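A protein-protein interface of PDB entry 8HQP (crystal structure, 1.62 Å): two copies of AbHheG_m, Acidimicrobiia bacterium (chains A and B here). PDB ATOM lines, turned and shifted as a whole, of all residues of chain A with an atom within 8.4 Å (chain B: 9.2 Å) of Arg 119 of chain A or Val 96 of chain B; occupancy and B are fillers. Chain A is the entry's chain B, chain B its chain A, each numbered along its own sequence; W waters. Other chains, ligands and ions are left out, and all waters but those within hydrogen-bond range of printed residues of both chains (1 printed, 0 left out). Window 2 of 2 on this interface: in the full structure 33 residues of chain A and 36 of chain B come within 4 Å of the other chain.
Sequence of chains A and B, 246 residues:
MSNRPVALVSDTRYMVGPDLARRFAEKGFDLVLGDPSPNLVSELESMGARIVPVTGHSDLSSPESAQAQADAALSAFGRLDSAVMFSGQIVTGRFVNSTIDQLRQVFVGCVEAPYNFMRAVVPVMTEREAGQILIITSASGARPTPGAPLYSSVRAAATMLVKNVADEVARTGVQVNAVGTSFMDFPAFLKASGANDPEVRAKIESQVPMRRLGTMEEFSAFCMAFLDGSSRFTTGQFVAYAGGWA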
ATOM      1  N   SER A  62       6.407  -0.300  -5.763  1.00  0.00           N
ATOM      2  CA  SER A  62       7.725  -0.471  -5.174  1.00  0.00           C
ATOM      3  C   SER A  62       8.824  -0.069  -6.146  1.00  0.00           C
ATOM      4  O   SER A  62       8.623  -0.078  -7.365  1.00  0.00           O
ATOM      5  CB  SER A  62       7.932  -1.931  -4.743  1.00  0.00           C
ATOM      6  OG  SER A  62       8.319  -2.724  -5.851  1.00  0.00           O
ATOM      7  N   PRO A  63      10.001   0.305  -5.635  1.00  0.00           N
ATOM      8  CA  PRO A  63      11.162   0.442  -6.528  1.00  0.00           C
ATOM      9  C   PRO A  63      11.438  -0.830  -7.303  1.00  0.00           C
ATOM     10  O   PRO A  63      11.869  -0.773  -8.463  1.00  0.00           O
ATOM     11  CB  PRO A  63      12.308   0.764  -5.559  1.00  0.00           C
ATOM     12  CG  PRO A  63      11.627   1.464  -4.423  1.00  0.00           C
ATOM     13  CD  PRO A  63      10.318   0.725  -4.258  1.00  0.00           C
ATOM     14  N   ALA A  66       9.283  -1.143 -10.627  1.00  0.00           N
ATOM     15  CA  ALA A  66       9.801  -0.368 -11.748  1.00  0.00           C
ATOM     16  C   ALA A  66      11.101  -0.959 -12.269  1.00  0.00           C
ATOM     17  O   ALA A  66      11.327  -1.012 -13.485  1.00  0.00           O
ATOM     18  CB  ALA A  66      10.006   1.085 -11.326  1.00  0.00           C
ATOM     19  N   GLN A  67      11.975  -1.391 -11.357  1.00  0.00           N
ATOM     20  CA  GLN A  67      13.232  -1.999 -11.767  1.00  0.00           C
ATOM     21  C   GLN A  67      12.981  -3.277 -12.557  1.00  0.00           C
ATOM     22  O   GLN A  67      13.682  -3.557 -13.536  1.00  0.00           O
ATOM     23  CB  GLN A  67      14.092  -2.280 -10.534  1.00  0.00           C
ATOM     24  CG  GLN A  67      15.567  -2.455 -10.821  1.00  0.00           C
ATOM     25  CD  GLN A  67      16.148  -1.293 -11.602  1.00  0.00           C
ATOM     26  OE1 GLN A  67      16.161  -0.157 -11.126  1.00  0.00           O
ATOM     27  NE2 GLN A  67      16.654  -1.575 -12.796  1.00  0.00           N
ATOM     28  N   ALA A  70      12.132  -2.292 -16.155  1.00  0.00           N
ATOM     29  CA  ALA A  70      13.330  -1.851 -16.865  1.00  0.00           C
ATOM     30  C   ALA A  70      14.281  -3.013 -17.131  1.00  0.00           C
ATOM     31  O   ALA A  70      14.877  -3.100 -18.212  1.00  0.00           O
ATOM     32  CB  ALA A  70      14.041  -0.752 -16.071  1.00  0.00           C
ATOM     33  N   GLU A 112       4.925   8.924  -5.976  1.00  0.00           N
ATOM     34  CA  GLU A 112       5.813   7.783  -5.757  1.00  0.00           C
ATOM     35  C   GLU A 112       5.899   6.904  -6.996  1.00  0.00           C
ATOM     36  O   GLU A 112       6.978   6.415  -7.344  1.00  0.00           O
ATOM     37  CB  GLU A 112       5.340   6.970  -4.558  1.00  0.00           C
ATOM     38  CG  GLU A 112       5.361   7.738  -3.246  1.00  0.00           C
ATOM     39  CD  GLU A 112       5.412   6.825  -2.033  1.00  0.00           C
ATOM     40  OE1 GLU A 112       5.388   5.588  -2.209  1.00  0.00           O
ATOM     41  OE2 GLU A 112       5.475   7.350  -0.901  1.00  0.00           O
ATOM     42  N   ALA A 113       4.769   6.667  -7.662  1.00  0.00           N
ATOM     43  CA  ALA A 113       4.796   5.837  -8.865  1.00  0.00           C
ATOM     44  C   ALA A 113       5.630   6.464  -9.974  1.00  0.00           C
ATOM     45  O   ALA A 113       6.496   5.765 -10.529  1.00  0.00           O
ATOM     46  CB  ALA A 113       3.364   5.520  -9.318  1.00  0.00           C
ATOM     47  N   PRO A 114       5.449   7.739 -10.346  1.00  0.00           N
ATOM     48  CA  PRO A 114       6.372   8.325 -11.331  1.00  0.00           C
ATOM     49  C   PRO A 114       7.809   8.383 -10.836  1.00  0.00           C
ATOM     50  O   PRO A 114       8.741   8.214 -11.636  1.00  0.00           O
ATOM     51  CB  PRO A 114       5.792   9.727 -11.562  1.00  0.00           C
ATOM     52  CG  PRO A 114       4.360   9.595 -11.220  1.00  0.00           C
ATOM     53  CD  PRO A 114       4.331   8.654 -10.051  1.00  0.00           C
ATOM     54  N   TYR A 115       8.023   8.622  -9.540  1.00  0.00           N
ATOM     55  CA  TYR A 115       9.386   8.581  -9.015  1.00  0.00           C
ATOM     56  C   TYR A 115      10.021   7.218  -9.271  1.00  0.00           C
ATOM     57  O   TYR A 115      11.127   7.127  -9.822  1.00  0.00           O
ATOM     58  CB  TYR A 115       9.408   8.903  -7.516  1.00  0.00           C
ATOM     59  CG  TYR A 115      10.788   8.692  -6.924  1.00  0.00           C
ATOM     60  CD1 TYR A 115      11.732   9.709  -6.948  1.00  0.00           C
ATOM     61  CD2 TYR A 115      11.169   7.459  -6.402  1.00  0.00           C
ATOM     62  CE1 TYR A 115      13.002   9.522  -6.437  1.00  0.00           C
ATOM     63  CE2 TYR A 115      12.437   7.258  -5.901  1.00  0.00           C
ATOM     64  CZ  TYR A 115      13.348   8.290  -5.924  1.00  0.00           C
ATOM     65  OH  TYR A 115      14.612   8.098  -5.429  1.00  0.00           O
ATOM     66  N   ASN A 116       9.323   6.144  -8.885  1.00  0.00           N
ATOM     67  CA  ASN A 116       9.874   4.801  -9.048  1.00  0.00           C
ATOM     68  C   ASN A 116      10.171   4.495 -10.508  1.00  0.00           C
ATOM     69  O   ASN A 116      11.230   3.939 -10.825  1.00  0.00           O
ATOM     70  CB  ASN A 116       8.912   3.757  -8.474  1.00  0.00           C
ATOM     71  CG  ASN A 116       8.862   3.785  -6.961  1.00  0.00           C
ATOM     72  OD1 ASN A 116       9.829   4.187  -6.307  1.00  0.00           O
ATOM     73  ND2 ASN A 116       7.735   3.353  -6.394  1.00  0.00           N
ATOM     74  N   PHE A 117       9.259   4.871 -11.410  1.00  0.00           N
ATOM     75  CA  PHE A 117       9.449   4.615 -12.835  1.00  0.00           C
ATOM     76  C   PHE A 117      10.708   5.301 -13.359  1.00  0.00           C
ATOM     77  O   PHE A 117      11.578   4.657 -13.956  1.00  0.00           O
ATOM     78  CB  PHE A 117       8.216   5.087 -13.609  1.00  0.00           C
ATOM     79  CG  PHE A 117       8.166   4.616 -15.038  1.00  0.00           C
ATOM     80  CD1 PHE A 117       7.910   3.287 -15.331  1.00  0.00           C
ATOM     81  CD2 PHE A 117       8.344   5.507 -16.084  1.00  0.00           C
ATOM     82  CE1 PHE A 117       7.842   2.850 -16.643  1.00  0.00           C
ATOM     83  CE2 PHE A 117       8.274   5.075 -17.408  1.00  0.00           C
ATOM     84  CZ  PHE A 117       8.025   3.743 -17.682  1.00  0.00           C
ATOM     85  N   MET A 118      10.834   6.608 -13.113  1.00  0.00           N
ATOM     86  CA  MET A 118      11.992   7.346 -13.605  1.00  0.00           C
ATOM     87  C   MET A 118      13.271   6.903 -12.906  1.00  0.00           C
ATOM     88  O   MET A 118      14.339   6.880 -13.525  1.00  0.00           O
ATOM     89  CB  MET A 118      11.788   8.851 -13.429  1.00  0.00           C
ATOM     90  CG  MET A 118      10.737   9.445 -14.369  1.00  0.00           C
ATOM     91  SD  MET A 118      10.609  11.240 -14.191  1.00  0.00           S
ATOM     92  CE  MET A 118       9.754  11.380 -12.617  1.00  0.00           C
ATOM     93  N   ARG A 119      13.188   6.566 -11.613  1.00  0.00           N
ATOM     94  CA  ARG A 119      14.375   6.133 -10.883  1.00  0.00           C
ATOM     95  C   ARG A 119      14.985   4.881 -11.497  1.00  0.00           C
ATOM     96  O   ARG A 119      16.209   4.705 -11.461  1.00  0.00           O
ATOM     97  CB  ARG A 119      14.024   5.880  -9.415  1.00  0.00           C
ATOM     98  CG  ARG A 119      15.224   5.763  -8.490  1.00  0.00           C
ATOM     99  CD  ARG A 119      16.216   6.907  -8.683  1.00  0.00           C
ATOM    100  NE  ARG A 119      17.418   6.733  -7.871  1.00  0.00           N
ATOM    101  CZ  ARG A 119      18.377   5.852  -8.118  1.00  0.00           C
ATOM    102  NH1 ARG A 119      18.438   5.202  -9.269  1.00  0.00           N
ATOM    103  NH2 ARG A 119      19.337   5.666  -7.213  1.00  0.00           N
ATOM    104  N   ALA A 120      14.148   4.002 -12.050  1.00  0.00           N
ATOM    105  CA  ALA A 120      14.623   2.798 -12.720  1.00  0.00           C
ATOM    106  C   ALA A 120      15.020   3.077 -14.167  1.00  0.00           C
ATOM    107  O   ALA A 120      16.067   2.616 -14.634  1.00  0.00           O
ATOM    108  CB  ALA A 120      13.543   1.714 -12.662  1.00  0.00           C
ATOM    109  N   VAL A 121      14.194   3.832 -14.891  1.00  0.00           N
ATOM    110  CA  VAL A 121      14.384   3.968 -16.332  1.00  0.00           C
ATOM    111  C   VAL A 121      15.506   4.947 -16.668  1.00  0.00           C
ATOM    112  O   VAL A 121      16.324   4.681 -17.561  1.00  0.00           O
ATOM    113  CB  VAL A 121      13.051   4.371 -16.991  1.00  0.00           C
ATOM    114  CG1 VAL A 121      13.255   4.669 -18.460  1.00  0.00           C
ATOM    115  CG2 VAL A 121      12.030   3.246 -16.827  1.00  0.00           C
ATOM    116  N   VAL A 122      15.577   6.082 -15.963  1.00  0.00           N
ATOM    117  CA  VAL A 122      16.545   7.120 -16.333  1.00  0.00           C
ATOM    118  C   VAL A 122      17.979   6.603 -16.357  1.00  0.00           C
ATOM    119  O   VAL A 122      18.699   6.895 -17.327  1.00  0.00           O
ATOM    120  CB  VAL A 122      16.381   8.351 -15.413  1.00  0.00           C
ATOM    121  CG1 VAL A 122      17.590   9.277 -15.546  1.00  0.00           C
ATOM    122  CG2 VAL A 122      15.106   9.108 -15.748  1.00  0.00           C
ATOM    123  N   PRO A 123      18.464   5.848 -15.359  1.00  0.00           N
ATOM    124  CA  PRO A 123      19.862   5.386 -15.438  1.00  0.00           C
ATOM    125  C   PRO A 123      20.135   4.510 -16.645  1.00  0.00           C
ATOM    126  O   PRO A 123      21.212   4.619 -17.242  1.00  0.00           O
ATOM    127  CB  PRO A 123      20.043   4.612 -14.129  1.00  0.00           C
ATOM    128  CG  PRO A 123      19.105   5.271 -13.192  1.00  0.00           C
ATOM    129  CD  PRO A 123      17.886   5.561 -14.031  1.00  0.00           C
ATOM    130  N   VAL A 124      19.178   3.663 -17.035  1.00  0.00           N
ATOM    131  CA  VAL A 124      19.344   2.854 -18.240  1.00  0.00           C
ATOM    132  C   VAL A 124      19.571   3.742 -19.452  1.00  0.00           C
ATOM    133  O   VAL A 124      20.435   3.465 -20.295  1.00  0.00           O
ATOM    134  CB  VAL A 124      18.118   1.941 -18.445  1.00  0.00           C
ATOM    135  CG1 VAL A 124      18.212   1.228 -19.788  1.00  0.00           C
ATOM    136  CG2 VAL A 124      17.997   0.937 -17.317  1.00  0.00           C
ATOM    137  N   THR A 126      20.480   7.133 -19.602  1.00  0.00           N
ATOM    138  CA  THR A 126      21.665   7.987 -19.617  1.00  0.00           C
ATOM    139  C   THR A 126      22.904   7.175 -19.961  1.00  0.00           C
ATOM    140  O   THR A 126      23.842   7.700 -20.570  1.00  0.00           O
ATOM    141  CB  THR A 126      21.849   8.709 -18.280  1.00  0.00           C
ATOM    142  OG1 THR A 126      22.020   7.750 -17.229  1.00  0.00           O
ATOM    143  CG2 THR A 126      20.654   9.604 -17.986  1.00  0.00           C
ATOM    144  N   ILE A 133      11.269   9.609 -22.273  1.00  0.00           N
ATOM    145  CA  ILE A 133      10.391   9.206 -21.181  1.00  0.00           C
ATOM    146  C   ILE A 133       9.210  10.154 -21.168  1.00  0.00           C
ATOM    147  O   ILE A 133       9.395  11.375 -21.238  1.00  0.00           O
ATOM    148  CB  ILE A 133      11.103   9.226 -19.817  1.00  0.00           C
ATOM    149  CG1 ILE A 133      12.270   8.248 -19.807  1.00  0.00           C
ATOM    150  CG2 ILE A 133      10.112   8.867 -18.701  1.00  0.00           C
ATOM    151  CD1 ILE A 133      13.236   8.486 -18.658  1.00  0.00           C
ATOM    152  N   ILE A 135       5.810  10.908 -18.756  1.00  0.00           N
ATOM    153  CA  ILE A 135       4.971  10.680 -17.585  1.00  0.00           C
ATOM    154  C   ILE A 135       3.600  11.248 -17.898  1.00  0.00           C
ATOM    155  O   ILE A 135       3.454  12.457 -18.106  1.00  0.00           O
ATOM    156  CB  ILE A 135       5.548  11.341 -16.322  1.00  0.00           C
ATOM    157  CG1 ILE A 135       6.966  10.841 -16.056  1.00  0.00           C
ATOM    158  CG2 ILE A 135       4.606  11.123 -15.122  1.00  0.00           C
ATOM    159  CD1 ILE A 135       7.071   9.330 -15.988  1.00  0.00           C
ATOM    160  N   LEU A 161       8.701  17.248 -10.332  1.00  0.00           N
ATOM    161  CA  LEU A 161       9.692  16.179 -10.321  1.00  0.00           C
ATOM    162  C   LEU A 161      10.187  15.893 -11.733  1.00  0.00           C
ATOM    163  O   LEU A 161      11.395  15.781 -11.970  1.00  0.00           O
ATOM    164  CB  LEU A 161       9.104  14.911  -9.701  1.00  0.00           C
ATOM    165  CG  LEU A 161      10.128  13.771  -9.643  1.00  0.00           C
ATOM    166  CD1 LEU A 161      11.365  14.203  -8.859  1.00  0.00           C
ATOM    167  CD2 LEU A 161       9.534  12.473  -9.096  1.00  0.00           C
ATOM    168  N   VAL A 165      14.033  16.188 -13.021  1.00  0.00           N
ATOM    169  CA  VAL A 165      14.757  15.084 -13.648  1.00  0.00           C
ATOM    170  C   VAL A 165      15.217  15.485 -15.041  1.00  0.00           C
ATOM    171  O   VAL A 165      16.363  15.228 -15.433  1.00  0.00           O
ATOM    172  CB  VAL A 165      13.876  13.820 -13.691  1.00  0.00           C
ATOM    173  CG1 VAL A 165      14.555  12.717 -14.496  1.00  0.00           C
ATOM    174  CG2 VAL A 165      13.558  13.338 -12.284  1.00  0.00           C
ATOM    175  N   GLU A 168      18.216  17.704 -14.890  1.00  0.00           N
ATOM    176  CA  GLU A 168      19.429  17.011 -14.465  1.00  0.00           C
ATOM    177  C   GLU A 168      20.087  16.252 -15.612  1.00  0.00           C
ATOM    178  O   GLU A 168      21.317  16.242 -15.727  1.00  0.00           O
ATOM    179  CB  GLU A 168      19.116  16.051 -13.314  1.00  0.00           C
ATOM    180  CG  GLU A 168      20.348  15.316 -12.770  1.00  0.00           C
ATOM    181  CD  GLU A 168      20.025  14.390 -11.605  1.00  0.00           C
ATOM    182  OE1 GLU A 168      19.432  14.879 -10.621  1.00  0.00           O
ATOM    183  OE2 GLU A 168      20.373  13.180 -11.672  1.00  0.00           O
ATOM    184  N   VAL A 169      19.294  15.612 -16.473  1.00  0.00           N
ATOM    185  CA  VAL A 169      19.840  14.741 -17.510  1.00  0.00           C
ATOM    186  C   VAL A 169      19.774  15.373 -18.895  1.00  0.00           C
ATOM    187  O   VAL A 169      19.993  14.683 -19.896  1.00  0.00           O
ATOM    188  CB  VAL A 169      19.156  13.364 -17.498  1.00  0.00           C
ATOM    189  CG1 VAL A 169      19.296  12.725 -16.125  1.00  0.00           C
ATOM    190  CG2 VAL A 169      17.689  13.483 -17.905  1.00  0.00           C
ATOM    191  N   THR A 172      22.585  14.607 -21.206  1.00  0.00           N
ATOM    192  CA  THR A 172      22.798  13.205 -21.567  1.00  0.00           C
ATOM    193  C   THR A 172      22.144  12.774 -22.875  1.00  0.00           C
ATOM    194  O   THR A 172      22.455  11.679 -23.358  1.00  0.00           O
ATOM    195  CB  THR A 172      22.263  12.279 -20.471  1.00  0.00           C
ATOM    196  OG1 THR A 172      20.831  12.368 -20.440  1.00  0.00           O
ATOM    197  CG2 THR A 172      22.837  12.641 -19.111  1.00  0.00           C
ATOM    198  N   GLY B  93      21.342  15.955  -3.592  1.00  0.00           N
ATOM    199  CA  GLY B  93      21.967  14.826  -4.256  1.00  0.00           C
ATOM    200  C   GLY B  93      21.259  14.681  -5.581  1.00  0.00           C
ATOM    201  O   GLY B  93      20.098  15.063  -5.737  1.00  0.00           O
ATOM    202  N   ARG B  94      21.962  14.106  -6.549  1.00  0.00           N
ATOM    203  CA  ARG B  94      21.373  13.941  -7.863  1.00  0.00           C
ATOM    204  C   ARG B  94      20.238  12.932  -7.821  1.00  0.00           C
ATOM    205  O   ARG B  94      20.215  12.008  -7.002  1.00  0.00           O
ATOM    206  CB  ARG B  94      22.422  13.509  -8.885  1.00  0.00           C
ATOM    207  CG  ARG B  94      23.299  14.658  -9.360  1.00  0.00           C
ATOM    208  CD  ARG B  94      24.466  14.166 -10.193  1.00  0.00           C
ATOM    209  NE  ARG B  94      24.908  12.839  -9.786  1.00  0.00           N
ATOM    210  CZ  ARG B  94      25.163  11.845 -10.624  1.00  0.00           C
ATOM    211  NH1 ARG B  94      25.049  11.997 -11.935  1.00  0.00           N
ATOM    212  NH2 ARG B  94      25.555  10.670 -10.137  1.00  0.00           N
ATOM    213  N   PHE B  95      19.285  13.128  -8.725  1.00  0.00           N
ATOM    214  CA  PHE B  95      18.123  12.254  -8.757  1.00  0.00           C
ATOM    215  C   PHE B  95      18.552  10.799  -8.907  1.00  0.00           C
ATOM    216  O   PHE B  95      18.003   9.909  -8.246  1.00  0.00           O
ATOM    217  CB  PHE B  95      17.205  12.665  -9.902  1.00  0.00           C
ATOM    218  CG  PHE B  95      16.109  11.685 -10.165  1.00  0.00           C
ATOM    219  CD1 PHE B  95      15.009  11.648  -9.332  1.00  0.00           C
ATOM    220  CD2 PHE B  95      16.183  10.792 -11.228  1.00  0.00           C
ATOM    221  CE1 PHE B  95      13.989  10.751  -9.547  1.00  0.00           C
ATOM    222  CE2 PHE B  95      15.163   9.888 -11.448  1.00  0.00           C
ATOM    223  CZ  PHE B  95      14.065   9.867 -10.602  1.00  0.00           C
ATOM    224  N   VAL B  96      19.549  10.545  -9.759  1.00  0.00           N
ATOM    225  CA  VAL B  96      19.986   9.185 -10.049  1.00  0.00           C
ATOM    226  C   VAL B  96      20.704   8.521  -8.881  1.00  0.00           C
ATOM    227  O   VAL B  96      20.996   7.323  -8.961  1.00  0.00           O
ATOM    228  CB  VAL B  96      20.880   9.154 -11.304  1.00  0.00           C
ATOM    229  CG1 VAL B  96      20.069   9.544 -12.541  1.00  0.00           C
ATOM    230  CG2 VAL B  96      22.097  10.059 -11.130  1.00  0.00           C
ATOM    231  N   ASN B  97      21.056   9.264  -7.830  1.00  0.00           N
ATOM    232  CA  ASN B  97      21.568   8.654  -6.608  1.00  0.00           C
ATOM    233  C   ASN B  97      20.543   8.635  -5.482  1.00  0.00           C
ATOM    234  O   ASN B  97      20.843   8.106  -4.412  1.00  0.00           O
ATOM    235  CB  ASN B  97      22.833   9.370  -6.102  1.00  0.00           C
ATOM    236  CG  ASN B  97      23.952   9.405  -7.126  1.00  0.00           C
ATOM    237  OD1 ASN B  97      24.731  10.355  -7.170  1.00  0.00           O
ATOM    238  ND2 ASN B  97      24.047   8.366  -7.945  1.00  0.00           N
ATOM    239  N   SER B  98      19.337   9.161  -5.702  1.00  0.00           N
ATOM    240  CA  SER B  98      18.353   9.323  -4.639  1.00  0.00           C
ATOM    241  C   SER B  98      17.602   8.013  -4.368  1.00  0.00           C
ATOM    242  O   SER B  98      17.761   7.013  -5.071  1.00  0.00           O
ATOM    243  CB  SER B  98      17.390  10.457  -4.992  1.00  0.00           C
ATOM    244  OG  SER B  98      16.534  10.089  -6.059  1.00  0.00           O
ATOM    245  N   THR B  99      16.801   8.017  -3.298  1.00  0.00           N
ATOM    246  CA  THR B  99      15.972   6.877  -2.911  1.00  0.00           C
ATOM    247  C   THR B  99      14.540   7.323  -2.636  1.00  0.00           C
ATOM    248  O   THR B  99      14.277   8.487  -2.334  1.00  0.00           O
ATOM    249  CB  THR B  99      16.507   6.172  -1.657  1.00  0.00           C
ATOM    250  OG1 THR B  99      16.137   6.934  -0.503  1.00  0.00           O
ATOM    251  CG2 THR B  99      18.016   6.034  -1.704  1.00  0.00           C
ATOM    252  N   ILE B 100      13.605   6.369  -2.728  1.00  0.00           N
ATOM    253  CA  ILE B 100      12.210   6.677  -2.412  1.00  0.00           C
ATOM    254  C   ILE B 100      12.063   7.126  -0.962  1.00  0.00           C
ATOM    255  O   ILE B 100      11.202   7.956  -0.645  1.00  0.00           O
ATOM    256  CB  ILE B 100      11.300   5.466  -2.726  1.00  0.00           C
ATOM    257  CG1 ILE B 100       9.823   5.814  -2.500  1.00  0.00           C
ATOM    258  CG2 ILE B 100      11.677   4.263  -1.881  1.00  0.00           C
ATOM    259  CD1 ILE B 100       9.145   6.441  -3.702  1.00  0.00           C
ATOM    260  N   ASP B 101      12.903   6.607  -0.061  1.00  0.00           N
ATOM    261  CA  ASP B 101      12.796   6.990   1.345  1.00  0.00           C
ATOM    262  C   ASP B 101      13.112   8.467   1.548  1.00  0.00           C
ATOM    263  O   ASP B 101      12.492   9.129   2.388  1.00  0.00           O
ATOM    264  CB  ASP B 101      13.702   6.100   2.191  1.00  0.00           C
ATOM    265  CG  ASP B 101      13.709   4.661   1.703  1.00  0.00           C
ATOM    266  OD1 ASP B 101      14.345   4.380   0.660  1.00  0.00           O
ATOM    267  OD2 ASP B 101      13.054   3.817   2.350  1.00  0.00           O
ATOM    268  N   GLN B 102      14.070   9.000   0.789  1.00  0.00           N
ATOM    269  CA  GLN B 102      14.359  10.429   0.855  1.00  0.00           C
ATOM    270  C   GLN B 102      13.170  11.245   0.363  1.00  0.00           C
ATOM    271  O   GLN B 102      12.864  12.309   0.913  1.00  0.00           O
ATOM    272  CB  GLN B 102      15.598  10.751   0.021  1.00  0.00           C
ATOM    273  CG  GLN B 102      16.879  10.154   0.573  1.00  0.00           C
ATOM    274  CD  GLN B 102      18.049  10.329  -0.367  1.00  0.00           C
ATOM    275  OE1 GLN B 102      17.900  10.223  -1.581  1.00  0.00           O
ATOM    276  NE2 GLN B 102      19.228  10.588   0.189  1.00  0.00           N
ATOM    277  N   LEU B 103      12.501  10.772  -0.690  1.00  0.00           N
ATOM    278  CA  LEU B 103      11.328  11.482  -1.186  1.00  0.00           C
ATOM    279  C   LEU B 103      10.245  11.538  -0.119  1.00  0.00           C
ATOM    280  O   LEU B 103       9.594  12.575   0.063  1.00  0.00           O
ATOM    281  CB  LEU B 103      10.813  10.820  -2.466  1.00  0.00           C
ATOM    282  CG  LEU B 103       9.523  11.387  -3.071  1.00  0.00           C
ATOM    283  CD1 LEU B 103       9.792  12.757  -3.679  1.00  0.00           C
ATOM    284  CD2 LEU B 103       8.954  10.433  -4.104  1.00  0.00           C
ATOM    285  N   PRO B 149      16.529  17.810  -6.429  1.00  0.00           N
ATOM    286  CA  PRO B 149      15.337  17.567  -7.264  1.00  0.00           C
ATOM    287  C   PRO B 149      14.127  17.086  -6.482  1.00  0.00           C
ATOM    288  O   PRO B 149      12.997  17.476  -6.802  1.00  0.00           O
ATOM    289  CB  PRO B 149      15.828  16.510  -8.266  1.00  0.00           C
ATOM    290  CG  PRO B 149      16.954  15.808  -7.554  1.00  0.00           C
ATOM    291  CD  PRO B 149      17.625  16.872  -6.744  1.00  0.00           C
ATOM    292  N   LEU B 150      14.328  16.226  -5.478  1.00  0.00           N
ATOM    293  CA  LEU B 150      13.208  15.693  -4.708  1.00  0.00           C
ATOM    294  C   LEU B 150      12.602  16.776  -3.830  1.00  0.00           C
ATOM    295  O   LEU B 150      11.374  16.916  -3.740  1.00  0.00           O
ATOM    296  CB  LEU B 150      13.687  14.529  -3.841  1.00  0.00           C
ATOM    297  CG  LEU B 150      13.674  13.117  -4.425  1.00  0.00           C
ATOM    298  CD1 LEU B 150      14.391  13.083  -5.766  1.00  0.00           C
ATOM    299  CD2 LEU B 150      14.332  12.138  -3.451  1.00  0.00           C
HETATM  300  O   HOH W   1      22.474  12.576 -13.241  1.00  0.00           O
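The guanidinium group (NH2) of Arg 94 of chain B lies within hydrogen-bond range of the side-chain amide oxygen (OD1) of Asn 97 of chain B.
The side-chain hydroxyl (OG) of Ser 98 of chain B is in hydrogen-bond range of the backbone carbonyl oxygen (O) of Phe 95 of chain B, at 2.6 Å.
OE1 of Gln 102 of chain B lies within hydrogen-bond range of N of Thr 99 of chain B.
Hydrophobic or aromatic side chains of chain A that line the printed part of chain B: Pro 63, Tyr 115, Met 118, Val 122 and Val 165.
Of the 13 printed residues of chain B, 9 touch a printed residue of chain A.
Hydrophobic or aromatic side chains of chain B within 4 Å of the printed part of chain A: Phe 95, Val 96, Ile 100, Leu 103 and Leu 150.
Among the printed residues, 19 pairs touch across the chains.
Arg 119 of chain A touches four residues of chain B.
No residue of chain B comes within 4 Å of Ala 120 of chain A.
Printed residues of chain B within 4 Å of Glu 168 of chain A: Arg 94 (3.5 Å), Phe 95 (2.6 Å) and Val 96 (3.4 Å).
Thr 172 of chain A touches none of the printed residues of chain B.
Val 96 of chain B touches just these residues of chain A: Arg 119 (2.9 Å), Val 122 (3.9 Å) and Glu 168 (3.4 Å).
Gln 102 of chain B touches none of the printed residues of chain A.
Printed residues of chain A within 4 Å of Leu 103 of chain B: Tyr 115 (3.8 Å).
Of the printed residues of chain A, Leu 150 of chain B touches Tyr 115 (3.9 Å).
The nearest residue of chain A that does not touch Val 96 of chain B is Pro 123 of chain A (4.4 Å).
The nearest printed residue of chain B that does not touch Val 122 of chain A is Phe 95 of chain B (4.4 Å).
Ile 100 of chain B touches Glu 112 of chain A (CD1 to CB, 3.9 Å).
CB of Tyr 115 of chain A touches CD2 of Leu 103 of chain B, 3.8 Å away.
CD1 of Leu 150 of chain B touches CE1 of Tyr 115 of chain A, at 3.9 Å.
Asn 116 of chain A touches Ile 100 of chain B.
Phe 95 of chain B touches Met 118 of chain A (CE2 to O, 3.7 Å).
CG1 of Val 96 of chain B touches CG1 of Val 122 of chain A, 3.9 Å away.
The guanidinium group (NE) of Arg 119 of chain A is in hydrogen-bond range of the backbone carbonyl oxygen (O) of Phe 95 of chain B (3.3 Å).
The side-chain carboxylate of Glu 168 of chain A is in hydrogen-bond range of the backbone NH of Phe 95 of chain B, at 2.6 Å.
O of Val 96 of chain B is in hydrogen-bond range of NH2 of Arg 119 of chain A (2.9 Å).
N of Val 96 of chain B is in hydrogen-bond range of OE2 of Glu 168 of chain A (3.4 Å).
OH of Tyr 115 of chain A is in hydrogen-bond range of OG of Ser 98 of chain B (2.8 Å).
The backbone carbonyl oxygen of Ser 98 of chain B sits at hydrogen-bond distance from the guanidinium group of Arg 119 of chain A.
N of Thr 99 of chain B lies close to OH of Tyr 115 of chain A (3.1 Å).
The backbone NH of Ile 100 of chain B is in hydrogen-bond range of the side-chain hydroxyl of Tyr 115 of chain A, at 3.4 Å.
No position is printed for both chains.
Of the 19 pairs that touch across the chains among the printed residues, none has its exchanged pair printed and touching as well.
Water W1 bridges the side-chain carboxylate of Glu 168 of chain A (2.7 Å) and the guanidinium group of Arg 94 of chain B (2.9 Å).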
